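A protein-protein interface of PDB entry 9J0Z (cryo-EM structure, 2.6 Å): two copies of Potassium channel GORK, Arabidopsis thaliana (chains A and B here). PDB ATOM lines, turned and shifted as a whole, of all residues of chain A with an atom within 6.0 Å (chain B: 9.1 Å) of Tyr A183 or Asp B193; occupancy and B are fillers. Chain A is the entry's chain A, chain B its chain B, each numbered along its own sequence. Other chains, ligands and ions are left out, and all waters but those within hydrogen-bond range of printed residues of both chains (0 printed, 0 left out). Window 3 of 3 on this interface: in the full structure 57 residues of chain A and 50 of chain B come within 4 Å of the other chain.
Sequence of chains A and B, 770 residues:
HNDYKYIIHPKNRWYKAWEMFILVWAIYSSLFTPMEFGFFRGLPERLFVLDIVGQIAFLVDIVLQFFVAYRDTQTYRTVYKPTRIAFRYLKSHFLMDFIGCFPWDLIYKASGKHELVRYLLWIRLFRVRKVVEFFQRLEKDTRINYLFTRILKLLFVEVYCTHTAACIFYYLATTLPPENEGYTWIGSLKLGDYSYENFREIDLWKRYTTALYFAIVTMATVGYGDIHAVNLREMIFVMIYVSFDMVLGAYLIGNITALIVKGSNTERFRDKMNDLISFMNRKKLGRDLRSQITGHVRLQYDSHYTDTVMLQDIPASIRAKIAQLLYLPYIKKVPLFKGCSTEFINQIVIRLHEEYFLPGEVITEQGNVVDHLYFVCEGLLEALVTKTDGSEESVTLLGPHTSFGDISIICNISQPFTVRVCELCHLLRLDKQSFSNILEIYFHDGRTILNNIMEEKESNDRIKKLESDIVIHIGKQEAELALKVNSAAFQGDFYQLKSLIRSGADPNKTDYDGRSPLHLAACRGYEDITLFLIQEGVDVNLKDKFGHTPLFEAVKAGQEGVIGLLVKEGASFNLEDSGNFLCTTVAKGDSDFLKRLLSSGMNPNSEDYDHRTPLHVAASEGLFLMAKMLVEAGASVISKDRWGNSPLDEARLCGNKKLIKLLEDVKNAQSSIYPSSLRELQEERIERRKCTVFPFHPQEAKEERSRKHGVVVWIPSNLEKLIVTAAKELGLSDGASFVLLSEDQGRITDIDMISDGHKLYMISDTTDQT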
ATOM      1  N   LEU A 176      -1.331 -23.957   5.790  1.00  0.00           N
ATOM      2  CA  LEU A 176      -1.351 -24.501   7.123  1.00  0.00           C
ATOM      3  C   LEU A 176      -2.241 -23.576   7.942  1.00  0.00           C
ATOM      4  O   LEU A 176      -2.171 -22.355   7.760  1.00  0.00           O
ATOM      5  CB  LEU A 176       0.052 -24.551   7.704  1.00  0.00           C
ATOM      6  CG  LEU A 176       0.925 -25.682   7.221  1.00  0.00           C
ATOM      7  CD1 LEU A 176       2.141 -25.709   8.006  1.00  0.00           C
ATOM      8  CD2 LEU A 176       0.223 -26.944   7.478  1.00  0.00           C
ATOM      9  N   ASN A 180      -1.160 -23.998  13.415  1.00  0.00           N
ATOM     10  CA  ASN A 180       0.090 -24.628  13.005  1.00  0.00           C
ATOM     11  C   ASN A 180       0.900 -23.635  12.189  1.00  0.00           C
ATOM     12  O   ASN A 180       1.129 -23.798  11.004  1.00  0.00           O
ATOM     13  CB  ASN A 180      -0.179 -25.881  12.196  1.00  0.00           C
ATOM     14  CG  ASN A 180      -1.270 -26.700  12.767  1.00  0.00           C
ATOM     15  OD1 ASN A 180      -1.435 -26.769  13.976  1.00  0.00           O
ATOM     16  ND2 ASN A 180      -2.035 -27.337  11.904  1.00  0.00           N
ATOM     17  N   GLU A 181       1.333 -22.590  12.852  1.00  0.00           N
ATOM     18  CA  GLU A 181       1.907 -21.444  12.182  1.00  0.00           C
ATOM     19  C   GLU A 181       3.389 -21.348  12.457  1.00  0.00           C
ATOM     20  O   GLU A 181       4.139 -20.844  11.632  1.00  0.00           O
ATOM     21  CB  GLU A 181       1.176 -20.193  12.632  1.00  0.00           C
ATOM     22  CG  GLU A 181       1.588 -18.981  11.986  1.00  0.00           C
ATOM     23  CD  GLU A 181       1.282 -17.801  12.802  1.00  0.00           C
ATOM     24  OE1 GLU A 181       1.913 -17.625  13.852  1.00  0.00           O
ATOM     25  OE2 GLU A 181       0.393 -17.049  12.390  1.00  0.00           O
ATOM     26  N   GLY A 182       3.842 -21.911  13.558  1.00  0.00           N
ATOM     27  CA  GLY A 182       5.255 -21.987  13.818  1.00  0.00           C
ATOM     28  C   GLY A 182       5.892 -23.154  13.118  1.00  0.00           C
ATOM     29  O   GLY A 182       7.061 -23.439  13.333  1.00  0.00           O
ATOM     30  N   TYR A 183       5.134 -23.847  12.290  1.00  0.00           N
ATOM     31  CA  TYR A 183       5.694 -24.844  11.408  1.00  0.00           C
ATOM     32  C   TYR A 183       5.585 -24.329   9.984  1.00  0.00           C
ATOM     33  O   TYR A 183       5.302 -25.083   9.063  1.00  0.00           O
ATOM     34  CB  TYR A 183       4.982 -26.175  11.597  1.00  0.00           C
ATOM     35  CG  TYR A 183       5.716 -27.361  11.040  1.00  0.00           C
ATOM     36  CD1 TYR A 183       7.082 -27.448  11.104  1.00  0.00           C
ATOM     37  CD2 TYR A 183       5.032 -28.381  10.423  1.00  0.00           C
ATOM     38  CE1 TYR A 183       7.731 -28.507  10.573  1.00  0.00           C
ATOM     39  CE2 TYR A 183       5.678 -29.437   9.895  1.00  0.00           C
ATOM     40  CZ  TYR A 183       7.021 -29.498   9.977  1.00  0.00           C
ATOM     41  OH  TYR A 183       7.666 -30.574   9.444  1.00  0.00           O
ATOM     42  N   THR A 184       5.781 -23.033   9.798  1.00  0.00           N
ATOM     43  CA  THR A 184       5.866 -22.427   8.485  1.00  0.00           C
ATOM     44  C   THR A 184       7.142 -21.623   8.424  1.00  0.00           C
ATOM     45  O   THR A 184       7.750 -21.336   9.445  1.00  0.00           O
ATOM     46  CB  THR A 184       4.725 -21.494   8.184  1.00  0.00           C
ATOM     47  OG1 THR A 184       4.601 -20.571   9.254  1.00  0.00           O
ATOM     48  CG2 THR A 184       3.460 -22.235   8.052  1.00  0.00           C
ATOM     49  N   TRP A 185       7.546 -21.269   7.220  1.00  0.00           N
ATOM     50  CA  TRP A 185       8.772 -20.525   7.055  1.00  0.00           C
ATOM     51  C   TRP A 185       8.683 -19.115   7.580  1.00  0.00           C
ATOM     52  O   TRP A 185       9.719 -18.537   7.885  1.00  0.00           O
ATOM     53  CB  TRP A 185       9.162 -20.484   5.593  1.00  0.00           C
ATOM     54  CG  TRP A 185       8.295 -19.664   4.719  1.00  0.00           C
ATOM     55  CD1 TRP A 185       7.229 -20.089   4.033  1.00  0.00           C
ATOM     56  CD2 TRP A 185       8.443 -18.284   4.402  1.00  0.00           C
ATOM     57  NE1 TRP A 185       6.684 -19.073   3.329  1.00  0.00           N
ATOM     58  CE2 TRP A 185       7.425 -17.949   3.539  1.00  0.00           C
ATOM     59  CE3 TRP A 185       9.336 -17.295   4.788  1.00  0.00           C
ATOM     60  CZ2 TRP A 185       7.273 -16.686   3.057  1.00  0.00           C
ATOM     61  CZ3 TRP A 185       9.186 -16.057   4.304  1.00  0.00           C
ATOM     62  CH2 TRP A 185       8.169 -15.756   3.454  1.00  0.00           C
ATOM     63  N   GLY A 187       5.884 -17.910   9.904  1.00  0.00           N
ATOM     64  CA  GLY A 187       5.438 -17.836  11.275  1.00  0.00           C
ATOM     65  C   GLY A 187       6.469 -18.249  12.283  1.00  0.00           C
ATOM     66  O   GLY A 187       6.323 -17.941  13.465  1.00  0.00           O
ATOM     67  N   SER A 188       7.510 -18.921  11.843  1.00  0.00           N
ATOM     68  CA  SER A 188       8.631 -19.287  12.677  1.00  0.00           C
ATOM     69  C   SER A 188       9.869 -18.495  12.325  1.00  0.00           C
ATOM     70  O   SER A 188      10.977 -18.999  12.457  1.00  0.00           O
ATOM     71  CB  SER A 188       8.920 -20.759  12.520  1.00  0.00           C
ATOM     72  OG  SER A 188       9.762 -20.911  11.420  1.00  0.00           O
ATOM     73  N   VAL A 230      10.795 -24.757   6.401  1.00  0.00           N
ATOM     74  CA  VAL A 230      10.684 -25.642   7.546  1.00  0.00           C
ATOM     75  C   VAL A 230       9.667 -26.741   7.343  1.00  0.00           C
ATOM     76  O   VAL A 230       9.791 -27.794   7.974  1.00  0.00           O
ATOM     77  CB  VAL A 230      10.382 -24.877   8.846  1.00  0.00           C
ATOM     78  CG1 VAL A 230      11.242 -23.695   8.955  1.00  0.00           C
ATOM     79  CG2 VAL A 230       9.004 -24.508   8.956  1.00  0.00           C
ATOM     80  N   ASN A 231       8.715 -26.590   6.449  1.00  0.00           N
ATOM     81  CA  ASN A 231       7.643 -27.533   6.224  1.00  0.00           C
ATOM     82  C   ASN A 231       8.165 -28.691   5.440  1.00  0.00           C
ATOM     83  O   ASN A 231       9.342 -28.813   5.188  1.00  0.00           O
ATOM     84  CB  ASN A 231       6.537 -26.908   5.412  1.00  0.00           C
ATOM     85  CG  ASN A 231       5.407 -26.540   6.203  1.00  0.00           C
ATOM     86  OD1 ASN A 231       5.091 -27.199   7.156  1.00  0.00           O
ATOM     87  ND2 ASN A 231       4.744 -25.481   5.816  1.00  0.00           N
ATOM     88  N   LEU A 232       7.261 -29.516   4.989  1.00  0.00           N
ATOM     89  CA  LEU A 232       7.585 -30.504   3.993  1.00  0.00           C
ATOM     90  C   LEU A 232       7.045 -30.122   2.639  1.00  0.00           C
ATOM     91  O   LEU A 232       7.547 -30.590   1.635  1.00  0.00           O
ATOM     92  CB  LEU A 232       7.030 -31.844   4.415  1.00  0.00           C
ATOM     93  CG  LEU A 232       7.845 -33.051   4.064  1.00  0.00           C
ATOM     94  CD1 LEU A 232       9.027 -33.003   4.931  1.00  0.00           C
ATOM     95  CD2 LEU A 232       7.015 -34.228   4.382  1.00  0.00           C
ATOM     96  N   GLU A 234       7.055 -26.899   1.737  1.00  0.00           N
ATOM     97  CA  GLU A 234       7.980 -25.858   1.354  1.00  0.00           C
ATOM     98  C   GLU A 234       9.334 -26.396   0.991  1.00  0.00           C
ATOM     99  O   GLU A 234      10.006 -25.797   0.160  1.00  0.00           O
ATOM    100  CB  GLU A 234       8.155 -24.861   2.479  1.00  0.00           C
ATOM    101  CG  GLU A 234       6.942 -24.131   2.805  1.00  0.00           C
ATOM    102  CD  GLU A 234       6.941 -23.685   4.211  1.00  0.00           C
ATOM    103  OE1 GLU A 234       8.024 -23.493   4.761  1.00  0.00           O
ATOM    104  OE2 GLU A 234       5.856 -23.570   4.791  1.00  0.00           O
ATOM    105  N   LEU B 189      18.346 -32.036  14.580  1.00  0.00           N
ATOM    106  CA  LEU B 189      17.709 -31.076  13.700  1.00  0.00           C
ATOM    107  C   LEU B 189      16.454 -30.537  14.349  1.00  0.00           C
ATOM    108  O   LEU B 189      15.733 -31.257  15.030  1.00  0.00           O
ATOM    109  CB  LEU B 189      17.362 -31.722  12.371  1.00  0.00           C
ATOM    110  CG  LEU B 189      16.922 -30.888  11.190  1.00  0.00           C
ATOM    111  CD1 LEU B 189      17.838 -29.777  11.030  1.00  0.00           C
ATOM    112  CD2 LEU B 189      16.948 -31.713   9.978  1.00  0.00           C
ATOM    113  N   LYS B 190      16.212 -29.251  14.147  1.00  0.00           N
ATOM    114  CA  LYS B 190      15.013 -28.583  14.626  1.00  0.00           C
ATOM    115  C   LYS B 190      14.628 -27.616  13.530  1.00  0.00           C
ATOM    116  O   LYS B 190      15.328 -26.630  13.324  1.00  0.00           O
ATOM    117  CB  LYS B 190      15.260 -27.823  15.916  1.00  0.00           C
ATOM    118  CG  LYS B 190      14.916 -28.531  17.177  1.00  0.00           C
ATOM    119  CD  LYS B 190      16.161 -29.130  17.766  1.00  0.00           C
ATOM    120  CE  LYS B 190      15.905 -29.851  19.060  1.00  0.00           C
ATOM    121  NZ  LYS B 190      17.015 -30.796  19.330  1.00  0.00           N
ATOM    122  N   LEU B 191      13.549 -27.881  12.823  1.00  0.00           N
ATOM    123  CA  LEU B 191      13.095 -26.988  11.773  1.00  0.00           C
ATOM    124  C   LEU B 191      11.735 -26.470  12.184  1.00  0.00           C
ATOM    125  O   LEU B 191      10.779 -27.237  12.254  1.00  0.00           O
ATOM    126  CB  LEU B 191      13.037 -27.702  10.436  1.00  0.00           C
ATOM    127  CG  LEU B 191      14.401 -27.884   9.808  1.00  0.00           C
ATOM    128  CD1 LEU B 191      14.265 -28.536   8.527  1.00  0.00           C
ATOM    129  CD2 LEU B 191      15.039 -26.576   9.588  1.00  0.00           C
ATOM    130  N   GLY B 192      11.642 -25.200  12.457  1.00  0.00           N
ATOM    131  CA  GLY B 192      10.402 -24.639  12.960  1.00  0.00           C
ATOM    132  C   GLY B 192      10.200 -25.037  14.400  1.00  0.00           C
ATOM    133  O   GLY B 192      11.089 -24.894  15.180  1.00  0.00           O
ATOM    134  N   ASP B 193       9.021 -25.548  14.723  1.00  0.00           N
ATOM    135  CA  ASP B 193       8.783 -26.088  16.050  1.00  0.00           C
ATOM    136  C   ASP B 193       8.826 -27.600  16.047  1.00  0.00           C
ATOM    137  O   ASP B 193       8.347 -28.230  16.984  1.00  0.00           O
ATOM    138  CB  ASP B 193       7.468 -25.583  16.646  1.00  0.00           C
ATOM    139  CG  ASP B 193       6.253 -25.872  15.795  1.00  0.00           C
ATOM    140  OD1 ASP B 193       6.308 -26.622  14.814  1.00  0.00           O
ATOM    141  OD2 ASP B 193       5.188 -25.326  16.128  1.00  0.00           O
ATOM    142  N   TYR B 194       9.385 -28.184  15.003  1.00  0.00           N
ATOM    143  CA  TYR B 194       9.465 -29.620  14.852  1.00  0.00           C
ATOM    144  C   TYR B 194      10.879 -30.079  15.130  1.00  0.00           C
ATOM    145  O   TYR B 194      11.816 -29.666  14.454  1.00  0.00           O
ATOM    146  CB  TYR B 194       9.064 -30.035  13.456  1.00  0.00           C
ATOM    147  CG  TYR B 194       8.979 -31.498  13.298  1.00  0.00           C
ATOM    148  CD1 TYR B 194       8.040 -32.214  13.987  1.00  0.00           C
ATOM    149  CD2 TYR B 194       9.841 -32.173  12.471  1.00  0.00           C
ATOM    150  CE1 TYR B 194       7.963 -33.557  13.861  1.00  0.00           C
ATOM    151  CE2 TYR B 194       9.772 -33.516  12.345  1.00  0.00           C
ATOM    152  CZ  TYR B 194       8.833 -34.200  13.036  1.00  0.00           C
ATOM    153  OH  TYR B 194       8.746 -35.551  12.912  1.00  0.00           O
ATOM    154  N   SER B 195      11.026 -30.929  16.124  1.00  0.00           N
ATOM    155  CA  SER B 195      12.289 -31.547  16.460  1.00  0.00           C
ATOM    156  C   SER B 195      12.369 -32.895  15.793  1.00  0.00           C
ATOM    157  O   SER B 195      11.449 -33.698  15.913  1.00  0.00           O
ATOM    158  CB  SER B 195      12.413 -31.739  17.943  1.00  0.00           C
ATOM    159  OG  SER B 195      13.713 -32.158  18.266  1.00  0.00           O
ATOM    160  N   TYR B 196      13.471 -33.167  15.116  1.00  0.00           N
ATOM    161  CA  TYR B 196      13.657 -34.476  14.509  1.00  0.00           C
ATOM    162  C   TYR B 196      14.366 -35.409  15.474  1.00  0.00           C
ATOM    163  O   TYR B 196      15.257 -36.135  15.107  1.00  0.00           O
ATOM    164  CB  TYR B 196      14.471 -34.358  13.238  1.00  0.00           C
ATOM    165  CG  TYR B 196      13.801 -33.905  11.993  1.00  0.00           C
ATOM    166  CD1 TYR B 196      13.519 -34.796  10.988  1.00  0.00           C
ATOM    167  CD2 TYR B 196      13.523 -32.578  11.786  1.00  0.00           C
ATOM    168  CE1 TYR B 196      12.940 -34.391   9.851  1.00  0.00           C
ATOM    169  CE2 TYR B 196      12.947 -32.164  10.652  1.00  0.00           C
ATOM    170  CZ  TYR B 196      12.666 -33.073   9.684  1.00  0.00           C
ATOM    171  OH  TYR B 196      12.081 -32.659   8.532  1.00  0.00           O
ATOM    172  N   GLU B 197      13.932 -35.415  16.714  1.00  0.00           N
ATOM    173  CA  GLU B 197      14.483 -36.333  17.684  1.00  0.00           C
ATOM    174  C   GLU B 197      13.809 -37.666  17.483  1.00  0.00           C
ATOM    175  O   GLU B 197      12.675 -37.735  17.008  1.00  0.00           O
ATOM    176  CB  GLU B 197      14.267 -35.830  19.105  1.00  0.00           C
ATOM    177  CG  GLU B 197      12.811 -35.776  19.511  1.00  0.00           C
ATOM    178  CD  GLU B 197      12.519 -34.765  20.583  1.00  0.00           C
ATOM    179  OE1 GLU B 197      13.461 -34.080  21.025  1.00  0.00           O
ATOM    180  OE2 GLU B 197      11.342 -34.644  20.974  1.00  0.00           O
ATOM    181  N   ILE B 202      10.377 -41.549  12.560  1.00  0.00           N
ATOM    182  CA  ILE B 202       9.730 -40.535  11.752  1.00  0.00           C
ATOM    183  C   ILE B 202       9.269 -41.256  10.498  1.00  0.00           C
ATOM    184  O   ILE B 202       9.861 -42.268  10.127  1.00  0.00           O
ATOM    185  CB  ILE B 202      10.707 -39.376  11.492  1.00  0.00           C
ATOM    186  CG1 ILE B 202      11.022 -38.688  12.807  1.00  0.00           C
ATOM    187  CG2 ILE B 202      10.178 -38.384  10.544  1.00  0.00           C
ATOM    188  CD1 ILE B 202      11.711 -37.389  12.709  1.00  0.00           C
ATOM    189  N   LYS B 206       8.868 -38.101   5.261  1.00  0.00           N
ATOM    190  CA  LYS B 206       9.482 -36.966   5.923  1.00  0.00           C
ATOM    191  C   LYS B 206      10.989 -37.086   5.996  1.00  0.00           C
ATOM    192  O   LYS B 206      11.690 -36.118   5.712  1.00  0.00           O
ATOM    193  CB  LYS B 206       8.910 -36.797   7.323  1.00  0.00           C
ATOM    194  CG  LYS B 206       9.400 -35.570   8.018  1.00  0.00           C
ATOM    195  CD  LYS B 206       8.649 -35.310   9.275  1.00  0.00           C
ATOM    196  CE  LYS B 206       7.459 -34.453   9.044  1.00  0.00           C
ATOM    197  NZ  LYS B 206       7.862 -33.050   8.890  1.00  0.00           N
ATOM    198  N   THR B 210      13.448 -34.705   3.828  1.00  0.00           N
ATOM    199  CA  THR B 210      14.425 -33.907   4.545  1.00  0.00           C
ATOM    200  C   THR B 210      15.840 -34.202   4.103  1.00  0.00           C
ATOM    201  O   THR B 210      16.648 -33.284   4.005  1.00  0.00           O
ATOM    202  CB  THR B 210      14.303 -34.170   6.019  1.00  0.00           C
ATOM    203  OG1 THR B 210      12.926 -34.209   6.358  1.00  0.00           O
ATOM    204  CG2 THR B 210      14.944 -33.098   6.778  1.00  0.00           C
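Of chain B, only Leu B191 (3.7 Å), Asp B193 (3.5 Å), Tyr B194 (3.5 Å) and Lys B206 (2.5 Å) come within 4 Å of Tyr A183.
Of chain A, only Gly A182 (3.2 Å) and Tyr A183 (3.5 Å) come within 4 Å of Asp B193.
No residue of chain B comes within 4 Å of Asn A231.
Printed residues of chain A within 4 Å of Gly B192: Gly A182 and Val A230.
Of the printed residues of chain A, Tyr B194 touches Tyr A183 (3.5 Å).
The nearest residue of chain B that does not touch Tyr A183 is Gly B192 (4.7 Å).
The nearest residue of chain A that does not touch Asp B193 is Ser A188 (5.3 Å).
Printed residues of chain A that touch a printed residue of chain B: Gly A182, Tyr A183, Val A230 and Leu A232.
Hydrophobic or aromatic side chains of chain A that line the printed part of chain B: Tyr A183, Val A230 and Leu A232.
Hydrophobic or aromatic side chains of chain B within 4 Å of the printed part of chain A: Tyr B194.
Among the printed residues, 9 pairs touch across the chains.
Among the printed residues, pairs that only touch across the chains: Gly A182 with Gly B192 (3.6 Å), Tyr A183 with Leu B191 (3.7 Å), Tyr A183 with Asp B193 (3.5 Å), Tyr A183 with Tyr B194 (3.5 Å), Val A230 with Leu B191 (3.9 Å), Val A230 with Gly B192 (3.8 Å) and Leu A232 with Lys B206 (3.99 Å).
No position is printed for both chains.
The backbone carbonyl oxygen (O) of Tyr A183 lies close to the side-chain amide oxygen (OD1) of Asn A231 (2.9 Å).
The backbone NH (N) of Val A230 is in hydrogen-bond range of the side-chain carboxylate (OE1) of Glu A234 (3.5 Å).
The backbone NH of Asp B193 sits at hydrogen-bond distance from the backbone carbonyl oxygen of Gly A182 (3.2 Å).
The side-chain amino group of Lys B206 sits at hydrogen-bond distance from the side-chain hydroxyl of Tyr A183 (2.5 Å).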
